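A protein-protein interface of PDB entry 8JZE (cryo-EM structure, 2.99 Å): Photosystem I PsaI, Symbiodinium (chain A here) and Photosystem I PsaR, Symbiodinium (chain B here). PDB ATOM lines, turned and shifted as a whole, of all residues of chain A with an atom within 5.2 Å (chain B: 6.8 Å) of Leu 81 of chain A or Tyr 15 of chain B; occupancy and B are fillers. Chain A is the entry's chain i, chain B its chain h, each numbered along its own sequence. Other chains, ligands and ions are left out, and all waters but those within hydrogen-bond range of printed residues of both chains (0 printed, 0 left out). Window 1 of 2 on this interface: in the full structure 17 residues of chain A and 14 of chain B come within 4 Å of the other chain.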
ATOM      1  N   ASP A  76     -19.131 -36.645 -15.411  1.00  0.00           N
ATOM      2  CA  ASP A  76     -17.969 -35.908 -14.923  1.00  0.00           C
ATOM      3  C   ASP A  76     -17.523 -34.859 -15.934  1.00  0.00           C
ATOM      4  O   ASP A  76     -17.200 -33.723 -15.563  1.00  0.00           O
ATOM      5  CB  ASP A  76     -16.826 -36.876 -14.613  1.00  0.00           C
ATOM      6  CG  ASP A  76     -15.600 -36.180 -14.046  1.00  0.00           C
ATOM      7  OD1 ASP A  76     -15.731 -35.048 -13.532  1.00  0.00           O
ATOM      8  OD2 ASP A  76     -14.500 -36.767 -14.119  1.00  0.00           O
ATOM      9  N   TYR A  77     -17.499 -35.222 -17.218  1.00  0.00           N
ATOM     10  CA  TYR A  77     -17.116 -34.272 -18.257  1.00  0.00           C
ATOM     11  C   TYR A  77     -18.068 -33.084 -18.289  1.00  0.00           C
ATOM     12  O   TYR A  77     -17.636 -31.926 -18.360  1.00  0.00           O
ATOM     13  CB  TYR A  77     -17.085 -34.977 -19.614  1.00  0.00           C
ATOM     14  CG  TYR A  77     -17.163 -34.048 -20.803  1.00  0.00           C
ATOM     15  CD1 TYR A  77     -16.034 -33.390 -21.270  1.00  0.00           C
ATOM     16  CD2 TYR A  77     -18.365 -33.840 -21.467  1.00  0.00           C
ATOM     17  CE1 TYR A  77     -16.101 -32.546 -22.356  1.00  0.00           C
ATOM     18  CE2 TYR A  77     -18.442 -32.997 -22.555  1.00  0.00           C
ATOM     19  CZ  TYR A  77     -17.307 -32.353 -22.995  1.00  0.00           C
ATOM     20  OH  TYR A  77     -17.377 -31.514 -24.078  1.00  0.00           O
ATOM     21  N   GLU A  78     -19.373 -33.354 -18.229  1.00  0.00           N
ATOM     22  CA  GLU A  78     -20.360 -32.280 -18.268  1.00  0.00           C
ATOM     23  C   GLU A  78     -20.260 -31.391 -17.036  1.00  0.00           C
ATOM     24  O   GLU A  78     -20.373 -30.165 -17.142  1.00  0.00           O
ATOM     25  CB  GLU A  78     -21.765 -32.868 -18.403  1.00  0.00           C
ATOM     26  CG  GLU A  78     -22.858 -31.837 -18.634  1.00  0.00           C
ATOM     27  CD  GLU A  78     -24.223 -32.468 -18.840  1.00  0.00           C
ATOM     28  OE1 GLU A  78     -24.335 -33.705 -18.701  1.00  0.00           O
ATOM     29  OE2 GLU A  78     -25.183 -31.730 -19.144  1.00  0.00           O
ATOM     30  N   LYS A  79     -20.050 -31.987 -15.859  1.00  0.00           N
ATOM     31  CA  LYS A  79     -19.914 -31.191 -14.643  1.00  0.00           C
ATOM     32  C   LYS A  79     -18.679 -30.304 -14.698  1.00  0.00           C
ATOM     33  O   LYS A  79     -18.733 -29.128 -14.320  1.00  0.00           O
ATOM     34  CB  LYS A  79     -19.860 -32.106 -13.418  1.00  0.00           C
ATOM     35  CG  LYS A  79     -19.498 -31.384 -12.130  1.00  0.00           C
ATOM     36  CD  LYS A  79     -19.289 -32.355 -10.982  1.00  0.00           C
ATOM     37  CE  LYS A  79     -18.756 -31.638  -9.751  1.00  0.00           C
ATOM     38  NZ  LYS A  79     -19.654 -30.530  -9.320  1.00  0.00           N
ATOM     39  N   GLY A  80     -17.553 -30.851 -15.162  1.00  0.00           N
ATOM     40  CA  GLY A  80     -16.354 -30.040 -15.290  1.00  0.00           C
ATOM     41  C   GLY A  80     -16.521 -28.916 -16.293  1.00  0.00           C
ATOM     42  O   GLY A  80     -16.070 -27.791 -16.059  1.00  0.00           O
ATOM     43  N   LEU A  81     -17.176 -29.202 -17.420  1.00  0.00           N
ATOM     44  CA  LEU A  81     -17.430 -28.162 -18.410  1.00  0.00           C
ATOM     45  C   LEU A  81     -18.327 -27.070 -17.844  1.00  0.00           C
ATOM     46  O   LEU A  81     -18.090 -25.880 -18.075  1.00  0.00           O
ATOM     47  CB  LEU A  81     -18.052 -28.775 -19.665  1.00  0.00           C
ATOM     48  CG  LEU A  81     -18.455 -27.807 -20.779  1.00  0.00           C
ATOM     49  CD1 LEU A  81     -17.261 -27.002 -21.247  1.00  0.00           C
ATOM     50  CD2 LEU A  81     -19.078 -28.561 -21.939  1.00  0.00           C
ATOM     51  N   GLU A  82     -19.365 -27.456 -17.096  1.00  0.00           N
ATOM     52  CA  GLU A  82     -20.257 -26.469 -16.499  1.00  0.00           C
ATOM     53  C   GLU A  82     -19.524 -25.615 -15.472  1.00  0.00           C
ATOM     54  O   GLU A  82     -19.721 -24.395 -15.414  1.00  0.00           O
ATOM     55  CB  GLU A  82     -21.460 -27.170 -15.868  1.00  0.00           C
ATOM     56  CG  GLU A  82     -22.586 -26.242 -15.439  1.00  0.00           C
ATOM     57  CD  GLU A  82     -23.858 -26.995 -15.086  1.00  0.00           C
ATOM     58  OE1 GLU A  82     -23.887 -28.231 -15.269  1.00  0.00           O
ATOM     59  OE2 GLU A  82     -24.827 -26.354 -14.629  1.00  0.00           O
ATOM     60  N   GLU A  83     -18.669 -26.239 -14.658  1.00  0.00           N
ATOM     61  CA  GLU A  83     -17.890 -25.483 -13.684  1.00  0.00           C
ATOM     62  C   GLU A  83     -16.948 -24.505 -14.376  1.00  0.00           C
ATOM     63  O   GLU A  83     -16.819 -23.352 -13.952  1.00  0.00           O
ATOM     64  CB  GLU A  83     -17.107 -26.441 -12.783  1.00  0.00           C
ATOM     65  CG  GLU A  83     -16.501 -25.800 -11.538  1.00  0.00           C
ATOM     66  CD  GLU A  83     -15.224 -25.029 -11.820  1.00  0.00           C
ATOM     67  OE1 GLU A  83     -14.511 -25.378 -12.786  1.00  0.00           O
ATOM     68  OE2 GLU A  83     -14.936 -24.071 -11.075  1.00  0.00           O
ATOM     69  N   ALA A  84     -16.282 -24.949 -15.443  1.00  0.00           N
ATOM     70  CA  ALA A  84     -15.368 -24.067 -16.162  1.00  0.00           C
ATOM     71  C   ALA A  84     -16.108 -22.935 -16.859  1.00  0.00           C
ATOM     72  O   ALA A  84     -15.572 -21.830 -16.982  1.00  0.00           O
ATOM     73  CB  ALA A  84     -14.548 -24.867 -17.172  1.00  0.00           C
ATOM     74  N   TRP A  85     -17.329 -23.189 -17.330  1.00  0.00           N
ATOM     75  CA  TRP A  85     -18.101 -22.130 -17.968  1.00  0.00           C
ATOM     76  C   TRP A  85     -18.663 -21.149 -16.949  1.00  0.00           C
ATOM     77  O   TRP A  85     -18.860 -19.972 -17.270  1.00  0.00           O
ATOM     78  CB  TRP A  85     -19.226 -22.736 -18.805  1.00  0.00           C
ATOM     79  CG  TRP A  85     -20.215 -21.736 -19.317  1.00  0.00           C
ATOM     80  CD1 TRP A  85     -21.521 -21.606 -18.943  1.00  0.00           C
ATOM     81  CD2 TRP A  85     -19.976 -20.720 -20.296  1.00  0.00           C
ATOM     82  NE1 TRP A  85     -22.111 -20.575 -19.633  1.00  0.00           N
ATOM     83  CE2 TRP A  85     -21.181 -20.014 -20.470  1.00  0.00           C
ATOM     84  CE3 TRP A  85     -18.859 -20.340 -21.045  1.00  0.00           C
ATOM     85  CZ2 TRP A  85     -21.302 -18.950 -21.360  1.00  0.00           C
ATOM     86  CZ3 TRP A  85     -18.980 -19.284 -21.927  1.00  0.00           C
ATOM     87  CH2 TRP A  85     -20.191 -18.601 -22.078  1.00  0.00           C
ATOM     88  N   GLU A  86     -18.932 -21.608 -15.724  1.00  0.00           N
ATOM     89  CA  GLU A  86     -19.457 -20.709 -14.700  1.00  0.00           C
ATOM     90  C   GLU A  86     -18.459 -19.610 -14.359  1.00  0.00           C
ATOM     91  O   GLU A  86     -18.838 -18.443 -14.209  1.00  0.00           O
ATOM     92  CB  GLU A  86     -19.838 -21.496 -13.447  1.00  0.00           C
ATOM     93  CG  GLU A  86     -21.174 -22.211 -13.548  1.00  0.00           C
ATOM     94  CD  GLU A  86     -22.329 -21.254 -13.773  1.00  0.00           C
ATOM     95  OE1 GLU A  86     -22.309 -20.147 -13.194  1.00  0.00           O
ATOM     96  OE2 GLU A  86     -23.253 -21.607 -14.534  1.00  0.00           O
ATOM     97  N   VAL A  97     -24.699 -24.514 -19.774  1.00  0.00           N
ATOM     98  CA  VAL A  97     -23.954 -25.458 -20.601  1.00  0.00           C
ATOM     99  C   VAL A  97     -24.887 -26.500 -21.201  1.00  0.00           C
ATOM    100  O   VAL A  97     -24.735 -26.893 -22.365  1.00  0.00           O
ATOM    101  CB  VAL A  97     -22.825 -26.108 -19.783  1.00  0.00           C
ATOM    102  CG1 VAL A  97     -22.203 -27.259 -20.552  1.00  0.00           C
ATOM    103  CG2 VAL A  97     -21.779 -25.079 -19.449  1.00  0.00           C
ATOM    104  N   LEU A 101     -25.215 -27.001 -25.229  1.00  0.00           N
ATOM    105  CA  LEU A 101     -24.830 -28.222 -25.928  1.00  0.00           C
ATOM    106  C   LEU A 101     -26.024 -28.851 -26.635  1.00  0.00           C
ATOM    107  O   LEU A 101     -25.888 -29.383 -27.744  1.00  0.00           O
ATOM    108  CB  LEU A 101     -24.197 -29.215 -24.953  1.00  0.00           C
ATOM    109  CG  LEU A 101     -22.880 -28.796 -24.295  1.00  0.00           C
ATOM    110  CD1 LEU A 101     -22.339 -29.907 -23.412  1.00  0.00           C
ATOM    111  CD2 LEU A 101     -21.860 -28.407 -25.345  1.00  0.00           C
ATOM    112  N   LEU B  10     -16.795 -16.839 -27.160  1.00  0.00           N
ATOM    113  CA  LEU B  10     -16.261 -17.103 -25.829  1.00  0.00           C
ATOM    114  C   LEU B  10     -16.615 -18.509 -25.365  1.00  0.00           C
ATOM    115  O   LEU B  10     -15.781 -19.202 -24.771  1.00  0.00           O
ATOM    116  CB  LEU B  10     -16.787 -16.065 -24.839  1.00  0.00           C
ATOM    117  CG  LEU B  10     -16.530 -16.346 -23.358  1.00  0.00           C
ATOM    118  CD1 LEU B  10     -15.047 -16.253 -23.046  1.00  0.00           C
ATOM    119  CD2 LEU B  10     -17.328 -15.401 -22.477  1.00  0.00           C
ATOM    120  N   PHE B  11     -17.852 -18.943 -25.617  1.00  0.00           N
ATOM    121  CA  PHE B  11     -18.218 -20.313 -25.271  1.00  0.00           C
ATOM    122  C   PHE B  11     -17.409 -21.312 -26.084  1.00  0.00           C
ATOM    123  O   PHE B  11     -17.015 -22.363 -25.570  1.00  0.00           O
ATOM    124  CB  PHE B  11     -19.712 -20.555 -25.476  1.00  0.00           C
ATOM    125  CG  PHE B  11     -20.156 -21.934 -25.063  1.00  0.00           C
ATOM    126  CD1 PHE B  11     -20.512 -22.196 -23.751  1.00  0.00           C
ATOM    127  CD2 PHE B  11     -20.203 -22.971 -25.984  1.00  0.00           C
ATOM    128  CE1 PHE B  11     -20.915 -23.461 -23.364  1.00  0.00           C
ATOM    129  CE2 PHE B  11     -20.604 -24.240 -25.604  1.00  0.00           C
ATOM    130  CZ  PHE B  11     -20.960 -24.484 -24.291  1.00  0.00           C
ATOM    131  N   GLU B  12     -17.168 -21.010 -27.362  1.00  0.00           N
ATOM    132  CA  GLU B  12     -16.312 -21.867 -28.178  1.00  0.00           C
ATOM    133  C   GLU B  12     -14.939 -22.016 -27.537  1.00  0.00           C
ATOM    134  O   GLU B  12     -14.419 -23.128 -27.401  1.00  0.00           O
ATOM    135  CB  GLU B  12     -16.169 -21.295 -29.591  1.00  0.00           C
ATOM    136  CG  GLU B  12     -17.470 -21.049 -30.334  1.00  0.00           C
ATOM    137  CD  GLU B  12     -17.952 -22.256 -31.101  1.00  0.00           C
ATOM    138  OE1 GLU B  12     -17.103 -23.041 -31.570  1.00  0.00           O
ATOM    139  OE2 GLU B  12     -19.183 -22.417 -31.236  1.00  0.00           O
ATOM    140  N   GLN B  13     -14.340 -20.893 -27.135  1.00  0.00           N
ATOM    141  CA  GLN B  13     -13.005 -20.929 -26.545  1.00  0.00           C
ATOM    142  C   GLN B  13     -12.998 -21.701 -25.233  1.00  0.00           C
ATOM    143  O   GLN B  13     -12.102 -22.516 -24.992  1.00  0.00           O
ATOM    144  CB  GLN B  13     -12.486 -19.506 -26.336  1.00  0.00           C
ATOM    145  CG  GLN B  13     -12.343 -18.708 -27.619  1.00  0.00           C
ATOM    146  CD  GLN B  13     -11.343 -19.323 -28.578  1.00  0.00           C
ATOM    147  OE1 GLN B  13     -11.689 -19.697 -29.698  1.00  0.00           O
ATOM    148  NE2 GLN B  13     -10.094 -19.426 -28.143  1.00  0.00           N
ATOM    149  N   VAL B  14     -13.996 -21.465 -24.377  1.00  0.00           N
ATOM    150  CA  VAL B  14     -14.064 -22.164 -23.094  1.00  0.00           C
ATOM    151  C   VAL B  14     -14.225 -23.663 -23.315  1.00  0.00           C
ATOM    152  O   VAL B  14     -13.525 -24.480 -22.701  1.00  0.00           O
ATOM    153  CB  VAL B  14     -15.209 -21.596 -22.236  1.00  0.00           C
ATOM    154  CG1 VAL B  14     -15.499 -22.517 -21.064  1.00  0.00           C
ATOM    155  CG2 VAL B  14     -14.857 -20.208 -21.740  1.00  0.00           C
ATOM    156  N   TYR B  15     -15.145 -24.044 -24.205  1.00  0.00           N
ATOM    157  CA  TYR B  15     -15.395 -25.454 -24.478  1.00  0.00           C
ATOM    158  C   TYR B  15     -14.150 -26.131 -25.029  1.00  0.00           C
ATOM    159  O   TYR B  15     -13.790 -27.230 -24.599  1.00  0.00           O
ATOM    160  CB  TYR B  15     -16.563 -25.592 -25.458  1.00  0.00           C
ATOM    161  CG  TYR B  15     -16.907 -27.017 -25.839  1.00  0.00           C
ATOM    162  CD1 TYR B  15     -16.233 -27.667 -26.868  1.00  0.00           C
ATOM    163  CD2 TYR B  15     -17.919 -27.704 -25.187  1.00  0.00           C
ATOM    164  CE1 TYR B  15     -16.546 -28.963 -27.220  1.00  0.00           C
ATOM    165  CE2 TYR B  15     -18.243 -28.998 -25.535  1.00  0.00           C
ATOM    166  CZ  TYR B  15     -17.551 -29.624 -26.551  1.00  0.00           C
ATOM    167  OH  TYR B  15     -17.866 -30.916 -26.902  1.00  0.00           O
ATOM    168  N   LEU B  16     -13.480 -25.491 -25.990  1.00  0.00           N
ATOM    169  CA  LEU B  16     -12.291 -26.096 -26.578  1.00  0.00           C
ATOM    170  C   LEU B  16     -11.166 -26.210 -25.559  1.00  0.00           C
ATOM    171  O   LEU B  16     -10.510 -27.253 -25.471  1.00  0.00           O
ATOM    172  CB  LEU B  16     -11.840 -25.295 -27.799  1.00  0.00           C
ATOM    173  CG  LEU B  16     -12.768 -25.352 -29.014  1.00  0.00           C
ATOM    174  CD1 LEU B  16     -12.230 -24.504 -30.150  1.00  0.00           C
ATOM    175  CD2 LEU B  16     -12.965 -26.785 -29.465  1.00  0.00           C
ATOM    176  N   GLN B  17     -10.939 -25.160 -24.765  1.00  0.00           N
ATOM    177  CA  GLN B  17      -9.866 -25.197 -23.779  1.00  0.00           C
ATOM    178  C   GLN B  17     -10.116 -26.275 -22.734  1.00  0.00           C
ATOM    179  O   GLN B  17      -9.180 -26.961 -22.306  1.00  0.00           O
ATOM    180  CB  GLN B  17      -9.713 -23.821 -23.125  1.00  0.00           C
ATOM    181  CG  GLN B  17      -8.505 -23.680 -22.207  1.00  0.00           C
ATOM    182  CD  GLN B  17      -8.780 -24.154 -20.794  1.00  0.00           C
ATOM    183  OE1 GLN B  17      -9.930 -24.211 -20.356  1.00  0.00           O
ATOM    184  NE2 GLN B  17      -7.723 -24.504 -20.071  1.00  0.00           N
ATOM    185  N   TYR B  18     -11.369 -26.442 -22.305  1.00  0.00           N
ATOM    186  CA  TYR B  18     -11.669 -27.483 -21.326  1.00  0.00           C
ATOM    187  C   TYR B  18     -11.560 -28.873 -21.940  1.00  0.00           C
ATOM    188  O   TYR B  18     -10.947 -29.777 -21.358  1.00  0.00           O
ATOM    189  CB  TYR B  18     -13.062 -27.270 -20.734  1.00  0.00           C
ATOM    190  CG  TYR B  18     -13.525 -28.427 -19.882  1.00  0.00           C
ATOM    191  CD1 TYR B  18     -13.078 -28.573 -18.576  1.00  0.00           C
ATOM    192  CD2 TYR B  18     -14.401 -29.381 -20.385  1.00  0.00           C
ATOM    193  CE1 TYR B  18     -13.492 -29.633 -17.795  1.00  0.00           C
ATOM    194  CE2 TYR B  18     -14.820 -30.442 -19.612  1.00  0.00           C
ATOM    195  CZ  TYR B  18     -14.363 -30.563 -18.319  1.00  0.00           C
ATOM    196  OH  TYR B  18     -14.780 -31.622 -17.548  1.00  0.00           O
ATOM    197  N   THR B  19     -12.149 -29.066 -23.123  1.00  0.00           N
ATOM    198  CA  THR B  19     -12.229 -30.402 -23.696  1.00  0.00           C
ATOM    199  C   THR B  19     -10.869 -30.891 -24.176  1.00  0.00           C
ATOM    200  O   THR B  19     -10.561 -32.078 -24.057  1.00  0.00           O
ATOM    201  CB  THR B  19     -13.247 -30.424 -24.835  1.00  0.00           C
ATOM    202  OG1 THR B  19     -14.498 -29.904 -24.367  1.00  0.00           O
ATOM    203  CG2 THR B  19     -13.464 -31.843 -25.327  1.00  0.00           C
ATOM    204  N   SER B  20     -10.037 -30.000 -24.723  1.00  0.00           N
ATOM    205  CA  SER B  20      -8.711 -30.425 -25.160  1.00  0.00           C
ATOM    206  C   SER B  20      -7.870 -30.907 -23.989  1.00  0.00           C
ATOM    207  O   SER B  20      -7.027 -31.795 -24.152  1.00  0.00           O
ATOM    208  CB  SER B  20      -8.007 -29.284 -25.892  1.00  0.00           C
ATOM    209  OG  SER B  20      -7.917 -28.136 -25.069  1.00  0.00           O
ATOM    210  N   GLU B  21      -8.078 -30.336 -22.803  1.00  0.00           N
ATOM    211  CA  GLU B  21      -7.407 -30.842 -21.613  1.00  0.00           C
ATOM    212  C   GLU B  21      -8.051 -32.129 -21.114  1.00  0.00           C
ATOM    213  O   GLU B  21      -7.355 -33.022 -20.621  1.00  0.00           O
ATOM    214  CB  GLU B  21      -7.417 -29.779 -20.514  1.00  0.00           C
ATOM    215  CG  GLU B  21      -6.501 -28.601 -20.790  1.00  0.00           C
ATOM    216  CD  GLU B  21      -5.043 -29.005 -20.854  1.00  0.00           C
ATOM    217  OE1 GLU B  21      -4.646 -29.917 -20.099  1.00  0.00           O
ATOM    218  OE2 GLU B  21      -4.297 -28.420 -21.666  1.00  0.00           O
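OH of Tyr 15 of chain B sits at hydrogen-bond distance from OH of Tyr 77 of chain A (2.9 Å). The side-chain hydroxyl (OH) of Tyr 18 of chain B lies within hydrogen-bond range of the backbone carbonyl oxygen (O) of Tyr 77 of chain A (3.0 Å). OH of Tyr 18 of chain B sits close to N of Leu 81 of chain A (3.4 Å). OG1 of Thr 19 of chain B sits at hydrogen-bond distance from OH of Tyr 77 of chain A, 3.3 Å away.
The backbone carbonyl oxygen (O) of Tyr 15 of chain B lies within hydrogen-bond range of the side-chain hydroxyl (OG1) of Thr 19 of chain B, at 2.8 Å.
O of Asp 76 of chain A touches OH of Tyr 18 of chain B (3.8 Å). OH of Tyr 18 of chain B touches CA of Gly 80 of chain A (3.2 Å). Tyr 15 of chain B touches Leu 81 of chain A. CZ3 of Trp 85 of chain A touches CA of Phe 11 of chain B, at 3.6 Å. Leu 101 of chain A touches Tyr 15 of chain B (CD2 to CE2, 3.7 Å).
Leu 81 of chain A touches just these residues of chain B: Tyr 15 (3.6 Å) and Tyr 18 (3.3 Å). Printed residues of chain A within 4 Å of Tyr 15 of chain B: Tyr 77 (2.9 Å), Leu 81 (3.6 Å) and Leu 101 (3.7 Å). Of the printed residues of chain B, Trp 85 of chain A touches Phe 11. Printed residues of chain B within 4 Å of Asp 76 of chain A: Tyr 18. Gln 17 of chain B touches none of the printed residues of chain A.
Hydrophobic or aromatic side chains of chain B within 4 Å of the printed part of chain A: Phe 11, Tyr 15 and Tyr 18. Of the 13 printed residues of chain A, 6 touch a printed residue of chain B. Among the printed residues, no Asp or Glu carboxylate lies within 4 Å of a Lys or Arg side-chain nitrogen of the other chain.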
